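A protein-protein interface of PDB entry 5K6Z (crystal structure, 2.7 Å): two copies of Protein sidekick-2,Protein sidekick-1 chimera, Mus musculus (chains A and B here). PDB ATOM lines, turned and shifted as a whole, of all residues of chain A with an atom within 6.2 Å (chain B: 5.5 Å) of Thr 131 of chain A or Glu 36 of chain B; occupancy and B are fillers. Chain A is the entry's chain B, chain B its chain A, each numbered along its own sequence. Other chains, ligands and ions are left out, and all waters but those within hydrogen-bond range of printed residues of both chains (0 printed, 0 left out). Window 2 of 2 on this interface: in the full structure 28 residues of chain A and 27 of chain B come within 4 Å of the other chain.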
ATOM      1  N   GLN A 129       2.903  23.859  22.073  1.00  0.00           N
ATOM      2  CA  GLN A 129       2.555  22.480  22.376  1.00  0.00           C
ATOM      3  C   GLN A 129       1.732  21.925  21.221  1.00  0.00           C
ATOM      4  O   GLN A 129       0.671  22.466  20.892  1.00  0.00           O
ATOM      5  CB  GLN A 129       1.777  22.404  23.683  1.00  0.00           C
ATOM      6  CG  GLN A 129       1.330  21.007  24.030  1.00  0.00           C
ATOM      7  CD  GLN A 129       0.342  20.982  25.174  1.00  0.00           C
ATOM      8  OE1 GLN A 129      -0.768  20.475  25.029  1.00  0.00           O
ATOM      9  NE2 GLN A 129       0.744  21.521  26.322  1.00  0.00           N
ATOM     10  N   VAL A 130       2.222  20.849  20.608  1.00  0.00           N
ATOM     11  CA  VAL A 130       1.668  20.298  19.376  1.00  0.00           C
ATOM     12  C   VAL A 130       1.131  18.905  19.667  1.00  0.00           C
ATOM     13  O   VAL A 130       1.880  18.028  20.112  1.00  0.00           O
ATOM     14  CB  VAL A 130       2.722  20.246  18.260  1.00  0.00           C
ATOM     15  CG1 VAL A 130       2.209  19.434  17.082  1.00  0.00           C
ATOM     16  CG2 VAL A 130       3.117  21.655  17.828  1.00  0.00           C
ATOM     17  N   THR A 131      -0.156  18.697  19.403  1.00  0.00           N
ATOM     18  CA  THR A 131      -0.788  17.390  19.536  1.00  0.00           C
ATOM     19  C   THR A 131      -1.235  16.906  18.162  1.00  0.00           C
ATOM     20  O   THR A 131      -1.882  17.653  17.418  1.00  0.00           O
ATOM     21  CB  THR A 131      -1.988  17.441  20.485  1.00  0.00           C
ATOM     22  OG1 THR A 131      -1.589  18.001  21.741  1.00  0.00           O
ATOM     23  CG2 THR A 131      -2.544  16.038  20.714  1.00  0.00           C
ATOM     24  N   TRP A 132      -0.892  15.662  17.832  1.00  0.00           N
ATOM     25  CA  TRP A 132      -1.281  15.065  16.561  1.00  0.00           C
ATOM     26  C   TRP A 132      -2.643  14.391  16.670  1.00  0.00           C
ATOM     27  O   TRP A 132      -2.974  13.790  17.696  1.00  0.00           O
ATOM     28  CB  TRP A 132      -0.235  14.051  16.097  1.00  0.00           C
ATOM     29  CG  TRP A 132       0.924  14.683  15.404  1.00  0.00           C
ATOM     30  CD1 TRP A 132       2.119  15.032  15.959  1.00  0.00           C
ATOM     31  CD2 TRP A 132       1.001  15.050  14.023  1.00  0.00           C
ATOM     32  NE1 TRP A 132       2.939  15.588  15.007  1.00  0.00           N
ATOM     33  CE2 TRP A 132       2.274  15.611  13.810  1.00  0.00           C
ATOM     34  CE3 TRP A 132       0.115  14.962  12.947  1.00  0.00           C
ATOM     35  CZ2 TRP A 132       2.684  16.077  12.565  1.00  0.00           C
ATOM     36  CZ3 TRP A 132       0.525  15.429  11.714  1.00  0.00           C
ATOM     37  CH2 TRP A 132       1.797  15.979  11.533  1.00  0.00           C
ATOM     38  N   PHE A 133      -3.428  14.502  15.599  1.00  0.00           N
ATOM     39  CA  PHE A 133      -4.776  13.954  15.543  1.00  0.00           C
ATOM     40  C   PHE A 133      -4.988  13.262  14.206  1.00  0.00           C
ATOM     41  O   PHE A 133      -4.421  13.666  13.188  1.00  0.00           O
ATOM     42  CB  PHE A 133      -5.854  15.038  15.699  1.00  0.00           C
ATOM     43  CG  PHE A 133      -5.917  15.661  17.060  1.00  0.00           C
ATOM     44  CD1 PHE A 133      -5.087  16.719  17.392  1.00  0.00           C
ATOM     45  CD2 PHE A 133      -6.835  15.211  17.996  1.00  0.00           C
ATOM     46  CE1 PHE A 133      -5.156  17.305  18.640  1.00  0.00           C
ATOM     47  CE2 PHE A 133      -6.911  15.791  19.247  1.00  0.00           C
ATOM     48  CZ  PHE A 133      -6.070  16.842  19.572  1.00  0.00           C
ATOM     49  N   LYS A 138      -6.969  11.228  18.864  1.00  0.00           N
ATOM     50  CA  LYS A 138      -5.651  11.685  19.285  1.00  0.00           C
ATOM     51  C   LYS A 138      -4.640  10.549  19.169  1.00  0.00           C
ATOM     52  O   LYS A 138      -4.937   9.401  19.508  1.00  0.00           O
ATOM     53  CB  LYS A 138      -5.721  12.206  20.722  1.00  0.00           C
ATOM     54  CG  LYS A 138      -4.401  12.518  21.380  1.00  0.00           C
ATOM     55  CD  LYS A 138      -4.648  13.017  22.796  1.00  0.00           C
ATOM     56  CE  LYS A 138      -5.671  14.143  22.792  1.00  0.00           C
ATOM     57  NZ  LYS A 138      -6.039  14.585  24.160  1.00  0.00           N
ATOM     58  N   ILE A 139      -3.444  10.879  18.691  1.00  0.00           N
ATOM     59  CA  ILE A 139      -2.445   9.884  18.308  1.00  0.00           C
ATOM     60  C   ILE A 139      -1.382   9.829  19.404  1.00  0.00           C
ATOM     61  O   ILE A 139      -0.653  10.819  19.597  1.00  0.00           O
ATOM     62  CB  ILE A 139      -1.828  10.209  16.943  1.00  0.00           C
ATOM     63  CG1 ILE A 139      -2.933  10.320  15.892  1.00  0.00           C
ATOM     64  CG2 ILE A 139      -0.819   9.146  16.550  1.00  0.00           C
ATOM     65  CD1 ILE A 139      -2.418  10.466  14.485  1.00  0.00           C
ATOM     66  N   ASN A 151       8.320  17.686  16.981  1.00  0.00           N
ATOM     67  CA  ASN A 151       6.904  17.389  16.782  1.00  0.00           C
ATOM     68  C   ASN A 151       6.615  16.725  15.443  1.00  0.00           C
ATOM     69  O   ASN A 151       5.462  16.705  14.997  1.00  0.00           O
ATOM     70  CB  ASN A 151       6.050  18.649  16.938  1.00  0.00           C
ATOM     71  CG  ASN A 151       6.089  19.195  18.349  1.00  0.00           C
ATOM     72  OD1 ASN A 151       6.011  18.443  19.324  1.00  0.00           O
ATOM     73  ND2 ASN A 151       6.220  20.511  18.468  1.00  0.00           N
ATOM     74  N   TYR A 167      -3.641  15.811  11.237  1.00  0.00           N
ATOM     75  CA  TYR A 167      -3.581  17.239  11.504  1.00  0.00           C
ATOM     76  C   TYR A 167      -3.148  17.459  12.945  1.00  0.00           C
ATOM     77  O   TYR A 167      -3.242  16.560  13.786  1.00  0.00           O
ATOM     78  CB  TYR A 167      -4.924  17.923  11.224  1.00  0.00           C
ATOM     79  CG  TYR A 167      -6.090  17.408  12.044  1.00  0.00           C
ATOM     80  CD1 TYR A 167      -6.734  16.218  11.715  1.00  0.00           C
ATOM     81  CD2 TYR A 167      -6.562  18.126  13.137  1.00  0.00           C
ATOM     82  CE1 TYR A 167      -7.806  15.754  12.460  1.00  0.00           C
ATOM     83  CE2 TYR A 167      -7.632  17.673  13.885  1.00  0.00           C
ATOM     84  CZ  TYR A 167      -8.251  16.489  13.543  1.00  0.00           C
ATOM     85  OH  TYR A 167      -9.318  16.038  14.292  1.00  0.00           O
ATOM     86  N   VAL A 168      -2.658  18.670  13.220  1.00  0.00           N
ATOM     87  CA  VAL A 168      -2.114  19.017  14.527  1.00  0.00           C
ATOM     88  C   VAL A 168      -2.943  20.126  15.152  1.00  0.00           C
ATOM     89  O   VAL A 168      -3.519  20.975  14.462  1.00  0.00           O
ATOM     90  CB  VAL A 168      -0.635  19.457  14.455  1.00  0.00           C
ATOM     91  CG1 VAL A 168       0.240  18.303  14.050  1.00  0.00           C
ATOM     92  CG2 VAL A 168      -0.470  20.620  13.494  1.00  0.00           C
ATOM     93  N   GLN A 169      -2.990  20.115  16.479  1.00  0.00           N
ATOM     94  CA  GLN A 169      -3.437  21.257  17.263  1.00  0.00           C
ATOM     95  C   GLN A 169      -2.216  21.865  17.942  1.00  0.00           C
ATOM     96  O   GLN A 169      -1.493  21.172  18.668  1.00  0.00           O
ATOM     97  CB  GLN A 169      -4.481  20.853  18.301  1.00  0.00           C
ATOM     98  CG  GLN A 169      -5.168  22.040  18.943  1.00  0.00           C
ATOM     99  CD  GLN A 169      -5.916  21.663  20.203  1.00  0.00           C
ATOM    100  OE1 GLN A 169      -5.480  20.791  20.959  1.00  0.00           O
ATOM    101  NE2 GLN A 169      -7.053  22.319  20.440  1.00  0.00           N
ATOM    102  N   ALA A 170      -1.977  23.144  17.689  1.00  0.00           N
ATOM    103  CA  ALA A 170      -0.899  23.885  18.322  1.00  0.00           C
ATOM    104  C   ALA A 170      -1.501  24.875  19.306  1.00  0.00           C
ATOM    105  O   ALA A 170      -2.399  25.643  18.946  1.00  0.00           O
ATOM    106  CB  ALA A 170      -0.047  24.613  17.282  1.00  0.00           C
ATOM    107  N   VAL B   9      -6.673   7.231  30.390  1.00  0.00           N
ATOM    108  CA  VAL B   9      -5.511   8.082  30.613  1.00  0.00           C
ATOM    109  C   VAL B   9      -5.876   9.113  31.681  1.00  0.00           C
ATOM    110  O   VAL B   9      -6.751   9.962  31.445  1.00  0.00           O
ATOM    111  CB  VAL B   9      -5.045   8.765  29.322  1.00  0.00           C
ATOM    112  CG1 VAL B   9      -3.866   9.678  29.615  1.00  0.00           C
ATOM    113  CG2 VAL B   9      -4.681   7.727  28.280  1.00  0.00           C
ATOM    114  N   PRO B  10      -5.248   9.082  32.853  1.00  0.00           N
ATOM    115  CA  PRO B  10      -5.526  10.093  33.877  1.00  0.00           C
ATOM    116  C   PRO B  10      -4.936  11.438  33.491  1.00  0.00           C
ATOM    117  O   PRO B  10      -4.030  11.513  32.645  1.00  0.00           O
ATOM    118  CB  PRO B  10      -4.844   9.521  35.128  1.00  0.00           C
ATOM    119  CG  PRO B  10      -4.645   8.069  34.838  1.00  0.00           C
ATOM    120  CD  PRO B  10      -4.399   8.000  33.370  1.00  0.00           C
ATOM    121  N   PRO B  11      -5.419  12.526  34.089  1.00  0.00           N
ATOM    122  CA  PRO B  11      -4.914  13.853  33.717  1.00  0.00           C
ATOM    123  C   PRO B  11      -3.469  14.050  34.142  1.00  0.00           C
ATOM    124  O   PRO B  11      -3.055  13.648  35.231  1.00  0.00           O
ATOM    125  CB  PRO B  11      -5.847  14.815  34.464  1.00  0.00           C
ATOM    126  CG  PRO B  11      -7.054  14.003  34.804  1.00  0.00           C
ATOM    127  CD  PRO B  11      -6.551  12.613  35.024  1.00  0.00           C
ATOM    128  N   TYR B  12      -2.702  14.674  33.257  1.00  0.00           N
ATOM    129  CA  TYR B  12      -1.330  15.064  33.536  1.00  0.00           C
ATOM    130  C   TYR B  12      -1.056  16.340  32.753  1.00  0.00           C
ATOM    131  O   TYR B  12      -1.877  16.780  31.945  1.00  0.00           O
ATOM    132  CB  TYR B  12      -0.346  13.945  33.175  1.00  0.00           C
ATOM    133  CG  TYR B  12      -0.209  13.712  31.689  1.00  0.00           C
ATOM    134  CD1 TYR B  12      -1.166  12.990  30.990  1.00  0.00           C
ATOM    135  CD2 TYR B  12       0.877  14.217  30.987  1.00  0.00           C
ATOM    136  CE1 TYR B  12      -1.048  12.780  29.632  1.00  0.00           C
ATOM    137  CE2 TYR B  12       1.008  14.012  29.628  1.00  0.00           C
ATOM    138  CZ  TYR B  12       0.044  13.291  28.955  1.00  0.00           C
ATOM    139  OH  TYR B  12       0.171  13.083  27.600  1.00  0.00           O
ATOM    140  N   PHE B  13       0.100  16.945  32.992  1.00  0.00           N
ATOM    141  CA  PHE B  13       0.431  18.217  32.368  1.00  0.00           C
ATOM    142  C   PHE B  13       1.522  18.022  31.327  1.00  0.00           C
ATOM    143  O   PHE B  13       2.572  17.442  31.621  1.00  0.00           O
ATOM    144  CB  PHE B  13       0.849  19.248  33.418  1.00  0.00           C
ATOM    145  CG  PHE B  13      -0.301  19.754  34.236  1.00  0.00           C
ATOM    146  CD1 PHE B  13      -1.092  20.797  33.773  1.00  0.00           C
ATOM    147  CD2 PHE B  13      -0.616  19.169  35.452  1.00  0.00           C
ATOM    148  CE1 PHE B  13      -2.168  21.258  34.515  1.00  0.00           C
ATOM    149  CE2 PHE B  13      -1.685  19.625  36.199  1.00  0.00           C
ATOM    150  CZ  PHE B  13      -2.466  20.670  35.728  1.00  0.00           C
ATOM    151  N   LYS B  14       1.255  18.491  30.107  1.00  0.00           N
ATOM    152  CA  LYS B  14       2.261  18.471  29.053  1.00  0.00           C
ATOM    153  C   LYS B  14       3.310  19.549  29.270  1.00  0.00           C
ATOM    154  O   LYS B  14       4.507  19.300  29.099  1.00  0.00           O
ATOM    155  CB  LYS B  14       1.596  18.656  27.690  1.00  0.00           C
ATOM    156  CG  LYS B  14       1.004  17.398  27.106  1.00  0.00           C
ATOM    157  CD  LYS B  14       1.561  17.136  25.719  1.00  0.00           C
ATOM    158  CE  LYS B  14       1.286  15.702  25.296  1.00  0.00           C
ATOM    159  NZ  LYS B  14       1.834  14.735  26.297  1.00  0.00           N
ATOM    160  N   MET B  34      -2.184  23.678  30.676  1.00  0.00           N
ATOM    161  CA  MET B  34      -1.637  22.850  29.598  1.00  0.00           C
ATOM    162  C   MET B  34      -1.672  21.377  30.007  1.00  0.00           C
ATOM    163  O   MET B  34      -0.650  20.708  30.175  1.00  0.00           O
ATOM    164  CB  MET B  34      -0.222  23.299  29.254  1.00  0.00           C
ATOM    165  CG  MET B  34      -0.104  24.780  28.964  1.00  0.00           C
ATOM    166  SD  MET B  34      -1.124  25.256  27.558  1.00  0.00           S
ATOM    167  CE  MET B  34      -0.182  24.574  26.201  1.00  0.00           C
ATOM    168  N   ALA B  35      -2.887  20.867  30.154  1.00  0.00           N
ATOM    169  CA  ALA B  35      -3.087  19.504  30.606  1.00  0.00           C
ATOM    170  C   ALA B  35      -3.480  18.596  29.449  1.00  0.00           C
ATOM    171  O   ALA B  35      -4.105  19.024  28.474  1.00  0.00           O
ATOM    172  CB  ALA B  35      -4.153  19.446  31.698  1.00  0.00           C
ATOM    173  N   GLU B  36      -3.096  17.332  29.573  1.00  0.00           N
ATOM    174  CA  GLU B  36      -3.452  16.281  28.638  1.00  0.00           C
ATOM    175  C   GLU B  36      -4.127  15.155  29.411  1.00  0.00           C
ATOM    176  O   GLU B  36      -3.968  15.031  30.630  1.00  0.00           O
ATOM    177  CB  GLU B  36      -2.209  15.769  27.890  1.00  0.00           C
ATOM    178  CG  GLU B  36      -2.502  14.871  26.703  1.00  0.00           C
ATOM    179  CD  GLU B  36      -3.512  15.481  25.750  1.00  0.00           C
ATOM    180  OE1 GLU B  36      -3.111  16.308  24.902  1.00  0.00           O
ATOM    181  OE2 GLU B  36      -4.711  15.141  25.857  1.00  0.00           O
ATOM    182  N   GLY B  37      -4.898  14.345  28.703  1.00  0.00           N
ATOM    183  CA  GLY B  37      -5.550  13.211  29.323  1.00  0.00           C
ATOM    184  C   GLY B  37      -6.685  12.710  28.454  1.00  0.00           C
ATOM    185  O   GLY B  37      -6.897  13.184  27.338  1.00  0.00           O
ATOM    186  N   SER B  38      -7.409  11.735  28.994  1.00  0.00           N
ATOM    187  CA  SER B  38      -8.573  11.207  28.297  1.00  0.00           C
ATOM    188  C   SER B  38      -9.681  12.251  28.264  1.00  0.00           C
ATOM    189  O   SER B  38     -10.045  12.824  29.296  1.00  0.00           O
ATOM    190  CB  SER B  38      -9.068   9.926  28.965  1.00  0.00           C
ATOM    191  OG  SER B  38      -8.395   8.799  28.437  1.00  0.00           O
ATOM    192  N   TRP B  39     -10.202  12.508  27.068  1.00  0.00           N
ATOM    193  CA  TRP B  39     -11.312  13.434  26.891  1.00  0.00           C
ATOM    194  C   TRP B  39     -12.590  12.836  27.465  1.00  0.00           C
ATOM    195  O   TRP B  39     -12.822  11.633  27.355  1.00  0.00           O
ATOM    196  CB  TRP B  39     -11.491  13.779  25.412  1.00  0.00           C
ATOM    197  CG  TRP B  39     -10.433  14.704  24.897  1.00  0.00           C
ATOM    198  CD1 TRP B  39      -9.311  15.121  25.559  1.00  0.00           C
ATOM    199  CD2 TRP B  39     -10.399  15.338  23.615  1.00  0.00           C
ATOM    200  NE1 TRP B  39      -8.581  15.973  24.766  1.00  0.00           N
ATOM    201  CE2 TRP B  39      -9.227  16.123  23.566  1.00  0.00           C
ATOM    202  CE3 TRP B  39     -11.244  15.319  22.501  1.00  0.00           C
ATOM    203  CZ2 TRP B  39      -8.881  16.880  22.449  1.00  0.00           C
ATOM    204  CZ3 TRP B  39     -10.899  16.070  21.392  1.00  0.00           C
ATOM    205  CH2 TRP B  39      -9.727  16.841  21.374  1.00  0.00           C
ATOM    206  N   LEU B  41     -11.737  16.716  29.109  1.00  0.00           N
ATOM    207  CA  LEU B  41     -11.016  17.392  30.177  1.00  0.00           C
ATOM    208  C   LEU B  41     -11.781  18.638  30.602  1.00  0.00           C
ATOM    209  O   LEU B  41     -12.285  19.385  29.759  1.00  0.00           O
ATOM    210  CB  LEU B  41      -9.605  17.780  29.732  1.00  0.00           C
ATOM    211  CG  LEU B  41      -8.664  16.652  29.311  1.00  0.00           C
ATOM    212  CD1 LEU B  41      -7.359  17.216  28.779  1.00  0.00           C
ATOM    213  CD2 LEU B  41      -8.403  15.722  30.480  1.00  0.00           C
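Printed residues of chain A that touch a printed residue of chain B: Gln 129, Thr 131, Phe 133 and Lys 138.
Hydrophobic or aromatic side chains of chain A within 4 Å of the printed part of chain B: Phe 133.
Of the 13 printed residues of chain B, 5 touch a printed residue of chain A.
Printed residues of chain B that touch a printed residue of chain A: Lys 14, Met 34, Glu 36, Gly 37 and Trp 39.
Hydrophobic or aromatic side chains of chain B within 4 Å of the printed part of chain A: Met 34 and Trp 39.
Among the printed residues, 7 pairs touch across the chains.
No position is printed for both chains.
OE1 of Glu 36 of chain B is in salt-bridge range of NZ of Lys 138 of chain A (3.5 Å).
The indole nitrogen (NE1) of Trp 39 of chain B lies close to the side-chain amino group (NZ) of Lys 138 of chain A (3.0 Å).
OH of Tyr 12 of chain B is in hydrogen-bond range of NZ of Lys 14 of chain B, 2.7 Å away.
The backbone NH (N) of Glu 36 of chain B is in hydrogen-bond range of the backbone carbonyl oxygen (O) of Tyr 12 of chain B (2.7 Å).
O of Met 34 of chain B sits at hydrogen-bond distance from N of Lys 14 of chain B (2.9 Å).
O of Thr 131 of chain A is in hydrogen-bond range of N of Gln 169 of chain A (2.9 Å).
The backbone carbonyl oxygen of Tyr 167 of chain A lies within hydrogen-bond range of the backbone NH of Phe 133 of chain A (2.7 Å).
Of chain B, only Glu 36 comes within 4 Å of Thr 131 of chain A.
Printed residues of chain A within 4 Å of Glu 36 of chain B: Thr 131 and Lys 138.
Of the printed residues of chain B, Phe 133 of chain A touches Trp 39 (3.7 Å).
Of the printed residues of chain B, Lys 138 of chain A touches Glu 36, Gly 37 and Trp 39.
Of the printed residues of chain A, Lys 14 of chain B touches Gln 129.
Of the printed residues of chain A, Met 34 of chain B touches Gln 129 (3.2 Å).
Val 9 of chain B touches none of the printed residues of chain A.
The nearest residue of chain A that does not touch Glu 36 of chain B is Gln 129 of chain A (4.8 Å).
The nearest printed residue of chain A that does not touch Gly 37 of chain B is Gln 129 of chain A (8.3 Å).
Among the printed residues, pairs that only touch across the chains: Gln 129 of chain A with Met 34 of chain B, Gln 129 of chain A with Lys 14 of chain B, Lys 138 of chain A with Gly 37 of chain B, Phe 133 of chain A with Trp 39 of chain B and Thr 131 of chain A with Glu 36 of chain B.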
